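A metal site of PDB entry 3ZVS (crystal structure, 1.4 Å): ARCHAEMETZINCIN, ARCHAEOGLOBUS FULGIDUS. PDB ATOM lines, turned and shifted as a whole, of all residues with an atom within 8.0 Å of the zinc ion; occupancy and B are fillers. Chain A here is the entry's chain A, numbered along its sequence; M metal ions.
The side-chain sulfur (SG) of Cys 154 is bound to the zinc ion (2.3 Å).
The side-chain sulfur (SG) of Cys 151 is bound to the zinc ion, at 2.3 Å.
SG of Cys 128 binds the zinc ion (2.3 Å).
The side-chain sulfur (SG) of Cys 132 is bound to the zinc ion (2.4 Å).
Four residues have an atom within 4 Å of the zinc ion: Cys 128, Cys 132, Cys 151 and Cys 154.
The nearest printed residue that does not touch the zinc ion is Asn 130 (4.2 Å).
The backbone NH (N) of Cys 128 is in hydrogen-bond range of the backbone carbonyl oxygen (O) of Met 134, at 3.1 Å.
N of Asn 130 sits close to SG of Cys 128, 3.4 Å away.
SG of Cys 151 sits close to ND2 of Asn 130 (3.4 Å).
The side-chain sulfur of Cys 151 lies close to the backbone NH of Glu 153 (3.5 Å).
SG of Cys 132 lies close to N of Met 134.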
ATOM      1  N   LEU A 125     -11.907 -30.658  -4.571  1.00  0.00           N
ATOM      2  CA  LEU A 125     -10.660 -30.485  -5.318  1.00  0.00           C
ATOM      3  C   LEU A 125      -9.756 -29.425  -4.713  1.00  0.00           C
ATOM      4  O   LEU A 125     -10.148 -28.279  -4.492  1.00  0.00           O
ATOM      5  CB  LEU A 125     -10.921 -30.115  -6.782  1.00  0.00           C
ATOM      6  CG  LEU A 125     -11.744 -31.131  -7.566  1.00  0.00           C
ATOM      7  CD1 LEU A 125     -12.074 -30.607  -8.944  1.00  0.00           C
ATOM      8  CD2 LEU A 125     -10.963 -32.425  -7.711  1.00  0.00           C
ATOM      9  N   LYS A 126      -8.522 -29.817  -4.431  1.00  0.00           N
ATOM     10  CA  LYS A 126      -7.470 -28.886  -4.050  1.00  0.00           C
ATOM     11  C   LYS A 126      -6.839 -28.227  -5.276  1.00  0.00           C
ATOM     12  O   LYS A 126      -7.144 -28.566  -6.421  1.00  0.00           O
ATOM     13  CB  LYS A 126      -6.383 -29.630  -3.262  1.00  0.00           C
ATOM     14  CG  LYS A 126      -6.911 -30.242  -1.985  1.00  0.00           C
ATOM     15  CD  LYS A 126      -5.801 -30.907  -1.150  1.00  0.00           C
ATOM     16  CE  LYS A 126      -6.402 -31.961  -0.216  1.00  0.00           C
ATOM     17  NZ  LYS A 126      -7.066 -33.105  -0.953  1.00  0.00           N
ATOM     18  N   HIS A 127      -6.004 -27.219  -5.055  1.00  0.00           N
ATOM     19  CA  HIS A 127      -5.297 -26.650  -6.187  1.00  0.00           C
ATOM     20  C   HIS A 127      -4.547 -27.699  -6.963  1.00  0.00           C
ATOM     21  O   HIS A 127      -3.971 -28.617  -6.399  1.00  0.00           O
ATOM     22  CB  HIS A 127      -4.382 -25.518  -5.744  1.00  0.00           C
ATOM     23  CG  HIS A 127      -5.149 -24.322  -5.328  1.00  0.00           C
ATOM     24  ND1 HIS A 127      -4.762 -23.471  -4.323  1.00  0.00           N
ATOM     25  CD2 HIS A 127      -6.343 -23.858  -5.764  1.00  0.00           C
ATOM     26  CE1 HIS A 127      -5.677 -22.529  -4.164  1.00  0.00           C
ATOM     27  NE2 HIS A 127      -6.638 -22.728  -5.040  1.00  0.00           N
ATOM     28  N   CYS A 128      -4.568 -27.510  -8.278  1.00  0.00           N
ATOM     29  CA  CYS A 128      -4.009 -28.453  -9.238  1.00  0.00           C
ATOM     30  C   CYS A 128      -2.898 -27.762 -10.015  1.00  0.00           C
ATOM     31  O   CYS A 128      -3.023 -26.607 -10.441  1.00  0.00           O
ATOM     32  CB  CYS A 128      -5.143 -28.801 -10.197  1.00  0.00           C
ATOM     33  SG  CYS A 128      -4.643 -30.058 -11.462  1.00  0.00           S
ATOM     34  N   SER A 129      -1.788 -28.457 -10.274  1.00  0.00           N
ATOM     35  CA  SER A 129      -0.715 -27.810 -11.027  1.00  0.00           C
ATOM     36  C   SER A 129      -0.785 -28.098 -12.526  1.00  0.00           C
ATOM     37  O   SER A 129       0.028 -27.623 -13.315  1.00  0.00           O
ATOM     38  CB  SER A 129       0.643 -28.225 -10.486  1.00  0.00           C
ATOM     39  OG  SER A 129       0.836 -29.584 -10.718  1.00  0.00           O
ATOM     40  N   ASN A 130      -1.819 -28.816 -12.940  1.00  0.00           N
ATOM     41  CA  ASN A 130      -1.963 -29.177 -14.351  1.00  0.00           C
ATOM     42  C   ASN A 130      -2.578 -28.041 -15.174  1.00  0.00           C
ATOM     43  O   ASN A 130      -2.873 -26.969 -14.630  1.00  0.00           O
ATOM     44  CB  ASN A 130      -2.824 -30.427 -14.487  1.00  0.00           C
ATOM     45  CG  ASN A 130      -2.292 -31.601 -13.727  1.00  0.00           C
ATOM     46  OD1 ASN A 130      -1.092 -31.691 -13.464  1.00  0.00           O
ATOM     47  ND2 ASN A 130      -3.185 -32.505 -13.370  1.00  0.00           N
ATOM     48  N   ASN A 131      -2.787 -28.277 -16.470  1.00  0.00           N
ATOM     49  CA  ASN A 131      -3.441 -27.326 -17.338  1.00  0.00           C
ATOM     50  C   ASN A 131      -4.912 -27.451 -17.003  1.00  0.00           C
ATOM     51  O   ASN A 131      -5.614 -28.285 -17.557  1.00  0.00           O
ATOM     52  CB  ASN A 131      -3.166 -27.750 -18.777  1.00  0.00           C
ATOM     53  CG  ASN A 131      -3.510 -26.689 -19.775  1.00  0.00           C
ATOM     54  OD1 ASN A 131      -4.329 -25.813 -19.514  1.00  0.00           O
ATOM     55  ND2 ASN A 131      -2.897 -26.760 -20.955  1.00  0.00           N
ATOM     56  N   CYS A 132      -5.379 -26.661 -16.040  1.00  0.00           N
ATOM     57  CA  CYS A 132      -6.602 -26.967 -15.315  1.00  0.00           C
ATOM     58  C   CYS A 132      -7.167 -25.692 -14.677  1.00  0.00           C
ATOM     59  O   CYS A 132      -6.416 -24.892 -14.147  1.00  0.00           O
ATOM     60  CB  CYS A 132      -6.293 -27.973 -14.203  1.00  0.00           C
ATOM     61  SG  CYS A 132      -7.759 -28.599 -13.323  1.00  0.00           S
ATOM     62  N   VAL A 133      -8.510 -25.608 -14.645  1.00  0.00           N
ATOM     63  CA  VAL A 133      -9.193 -24.493 -13.966  1.00  0.00           C
ATOM     64  C   VAL A 133      -8.907 -24.473 -12.466  1.00  0.00           C
ATOM     65  O   VAL A 133      -9.053 -23.423 -11.845  1.00  0.00           O
ATOM     66  CB  VAL A 133     -10.706 -24.620 -14.249  1.00  0.00           C
ATOM     67  CG1 VAL A 133     -11.322 -25.831 -13.555  1.00  0.00           C
ATOM     68  CG2 VAL A 133     -11.439 -23.338 -13.897  1.00  0.00           C
ATOM     69  N   MET A 134      -8.520 -25.611 -11.883  1.00  0.00           N
ATOM     70  CA  MET A 134      -8.162 -25.680 -10.479  1.00  0.00           C
ATOM     71  C   MET A 134      -6.778 -25.168 -10.126  1.00  0.00           C
ATOM     72  O   MET A 134      -6.414 -25.153  -8.944  1.00  0.00           O
ATOM     73  CB  MET A 134      -8.375 -27.110  -9.891  1.00  0.00           C
ATOM     74  CG  MET A 134      -9.864 -27.554  -9.803  1.00  0.00           C
ATOM     75  SD  MET A 134     -10.976 -26.335  -9.035  1.00  0.00           S
ATOM     76  CE  MET A 134     -10.170 -26.076  -7.422  1.00  0.00           C
ATOM     77  N   ARG A 135      -6.010 -24.696 -11.102  1.00  0.00           N
ATOM     78  CA  ARG A 135      -4.769 -23.984 -10.757  1.00  0.00           C
ATOM     79  C   ARG A 135      -5.090 -22.791  -9.900  1.00  0.00           C
ATOM     80  O   ARG A 135      -6.059 -22.042 -10.167  1.00  0.00           O
ATOM     81  CB  ARG A 135      -4.108 -23.409 -12.005  1.00  0.00           C
ATOM     82  CG  ARG A 135      -3.357 -24.359 -12.882  1.00  0.00           C
ATOM     83  CD  ARG A 135      -2.536 -23.488 -13.875  1.00  0.00           C
ATOM     84  NE  ARG A 135      -2.112 -24.231 -15.065  1.00  0.00           N
ATOM     85  CZ  ARG A 135      -1.863 -23.678 -16.235  1.00  0.00           C
ATOM     86  NH1 ARG A 135      -2.015 -22.368 -16.438  1.00  0.00           N
ATOM     87  NH2 ARG A 135      -1.448 -24.464 -17.223  1.00  0.00           N
ATOM     88  N   SER A 149     -11.779 -25.558 -18.133  1.00  0.00           N
ATOM     89  CA  SER A 149     -12.116 -26.950 -17.955  1.00  0.00           C
ATOM     90  C   SER A 149     -11.242 -27.609 -16.897  1.00  0.00           C
ATOM     91  O   SER A 149     -10.074 -27.233 -16.644  1.00  0.00           O
ATOM     92  CB  SER A 149     -11.931 -27.702 -19.264  1.00  0.00           C
ATOM     93  OG  SER A 149     -10.666 -27.415 -19.772  1.00  0.00           O
ATOM     94  N   PHE A 150     -11.809 -28.613 -16.278  1.00  0.00           N
ATOM     95  CA  PHE A 150     -11.040 -29.475 -15.370  1.00  0.00           C
ATOM     96  C   PHE A 150     -10.151 -30.384 -16.200  1.00  0.00           C
ATOM     97  O   PHE A 150     -10.581 -30.911 -17.232  1.00  0.00           O
ATOM     98  CB  PHE A 150     -11.961 -30.350 -14.528  1.00  0.00           C
ATOM     99  CG  PHE A 150     -12.812 -29.559 -13.571  1.00  0.00           C
ATOM    100  CD1 PHE A 150     -12.276 -29.063 -12.397  1.00  0.00           C
ATOM    101  CD2 PHE A 150     -14.142 -29.298 -13.863  1.00  0.00           C
ATOM    102  CE1 PHE A 150     -13.040 -28.319 -11.518  1.00  0.00           C
ATOM    103  CE2 PHE A 150     -14.912 -28.561 -12.973  1.00  0.00           C
ATOM    104  CZ  PHE A 150     -14.363 -28.065 -11.810  1.00  0.00           C
ATOM    105  N   CYS A 151      -8.935 -30.578 -15.717  1.00  0.00           N
ATOM    106  CA  CYS A 151      -8.048 -31.586 -16.295  1.00  0.00           C
ATOM    107  C   CYS A 151      -8.630 -32.966 -16.074  1.00  0.00           C
ATOM    108  O   CYS A 151      -9.560 -33.170 -15.296  1.00  0.00           O
ATOM    109  CB  CYS A 151      -6.627 -31.497 -15.712  1.00  0.00           C
ATOM    110  SG  CYS A 151      -6.463 -32.125 -14.017  1.00  0.00           S
ATOM    111  N   ARG A 152      -8.061 -33.951 -16.774  1.00  0.00           N
ATOM    112  CA  ARG A 152      -8.576 -35.307 -16.670  1.00  0.00           C
ATOM    113  C   ARG A 152      -8.483 -35.868 -15.250  1.00  0.00           C
ATOM    114  O   ARG A 152      -9.331 -36.613 -14.808  1.00  0.00           O
ATOM    115  CB  ARG A 152      -7.849 -36.258 -17.656  1.00  0.00           C
ATOM    116  CG  ARG A 152      -8.031 -35.878 -19.097  1.00  0.00           C
ATOM    117  CD  ARG A 152      -7.372 -36.874 -20.066  1.00  0.00           C
ATOM    118  NE  ARG A 152      -5.914 -36.777 -20.089  1.00  0.00           N
ATOM    119  CZ  ARG A 152      -5.061 -37.671 -19.590  1.00  0.00           C
ATOM    120  NH1 ARG A 152      -5.483 -38.741 -18.974  1.00  0.00           N
ATOM    121  NH2 ARG A 152      -3.742 -37.439 -19.681  1.00  0.00           N
ATOM    122  N   GLU A 153      -7.449 -35.474 -14.513  1.00  0.00           N
ATOM    123  CA  GLU A 153      -7.336 -35.921 -13.145  1.00  0.00           C
ATOM    124  C   GLU A 153      -8.464 -35.360 -12.272  1.00  0.00           C
ATOM    125  O   GLU A 153      -9.079 -36.090 -11.520  1.00  0.00           O
ATOM    126  CB  GLU A 153      -5.981 -35.551 -12.548  1.00  0.00           C
ATOM    127  CG  GLU A 153      -4.864 -36.367 -13.178  1.00  0.00           C
ATOM    128  CD  GLU A 153      -3.572 -36.225 -12.433  1.00  0.00           C
ATOM    129  OE1 GLU A 153      -3.273 -35.096 -11.963  1.00  0.00           O
ATOM    130  OE2 GLU A 153      -2.848 -37.253 -12.313  1.00  0.00           O
ATOM    131  N   CYS A 154      -8.698 -34.060 -12.358  1.00  0.00           N
ATOM    132  CA  CYS A 154      -9.723 -33.460 -11.514  1.00  0.00           C
ATOM    133  C   CYS A 154     -11.101 -33.901 -11.918  1.00  0.00           C
ATOM    134  O   CYS A 154     -11.966 -34.144 -11.065  1.00  0.00           O
ATOM    135  CB  CYS A 154      -9.609 -31.949 -11.602  1.00  0.00           C
ATOM    136  SG  CYS A 154      -8.190 -31.258 -10.721  1.00  0.00           S
ATOM    137  N   ALA A 155     -11.314 -34.053 -13.224  1.00  0.00           N
ATOM    138  CA  ALA A 155     -12.622 -34.498 -13.725  1.00  0.00           C
ATOM    139  C   ALA A 155     -12.940 -35.889 -13.187  1.00  0.00           C
ATOM    140  O   ALA A 155     -14.093 -36.172 -12.850  1.00  0.00           O
ATOM    141  CB  ALA A 155     -12.659 -34.460 -15.208  1.00  0.00           C
ATOM    142  N   LYS A 157     -12.257 -37.119 -10.401  1.00  0.00           N
ATOM    143  CA  LYS A 157     -12.495 -37.083  -8.954  1.00  0.00           C
ATOM    144  C   LYS A 157     -13.861 -36.497  -8.581  1.00  0.00           C
ATOM    145  O   LYS A 157     -14.307 -36.611  -7.436  1.00  0.00           O
ATOM    146  CB  LYS A 157     -11.399 -36.249  -8.285  1.00  0.00           C
ATOM    147  CG  LYS A 157     -10.002 -36.855  -8.249  1.00  0.00           C
ATOM    148  CD  LYS A 157      -9.050 -35.800  -7.668  1.00  0.00           C
ATOM    149  CE  LYS A 157      -7.666 -36.314  -7.350  1.00  0.00           C
ATOM    150  NZ  LYS A 157      -6.849 -36.412  -8.558  1.00  0.00           N
HETATM  151 ZN    ZN M   1      -6.749 -30.513 -12.372  1.00  0.00          ZN
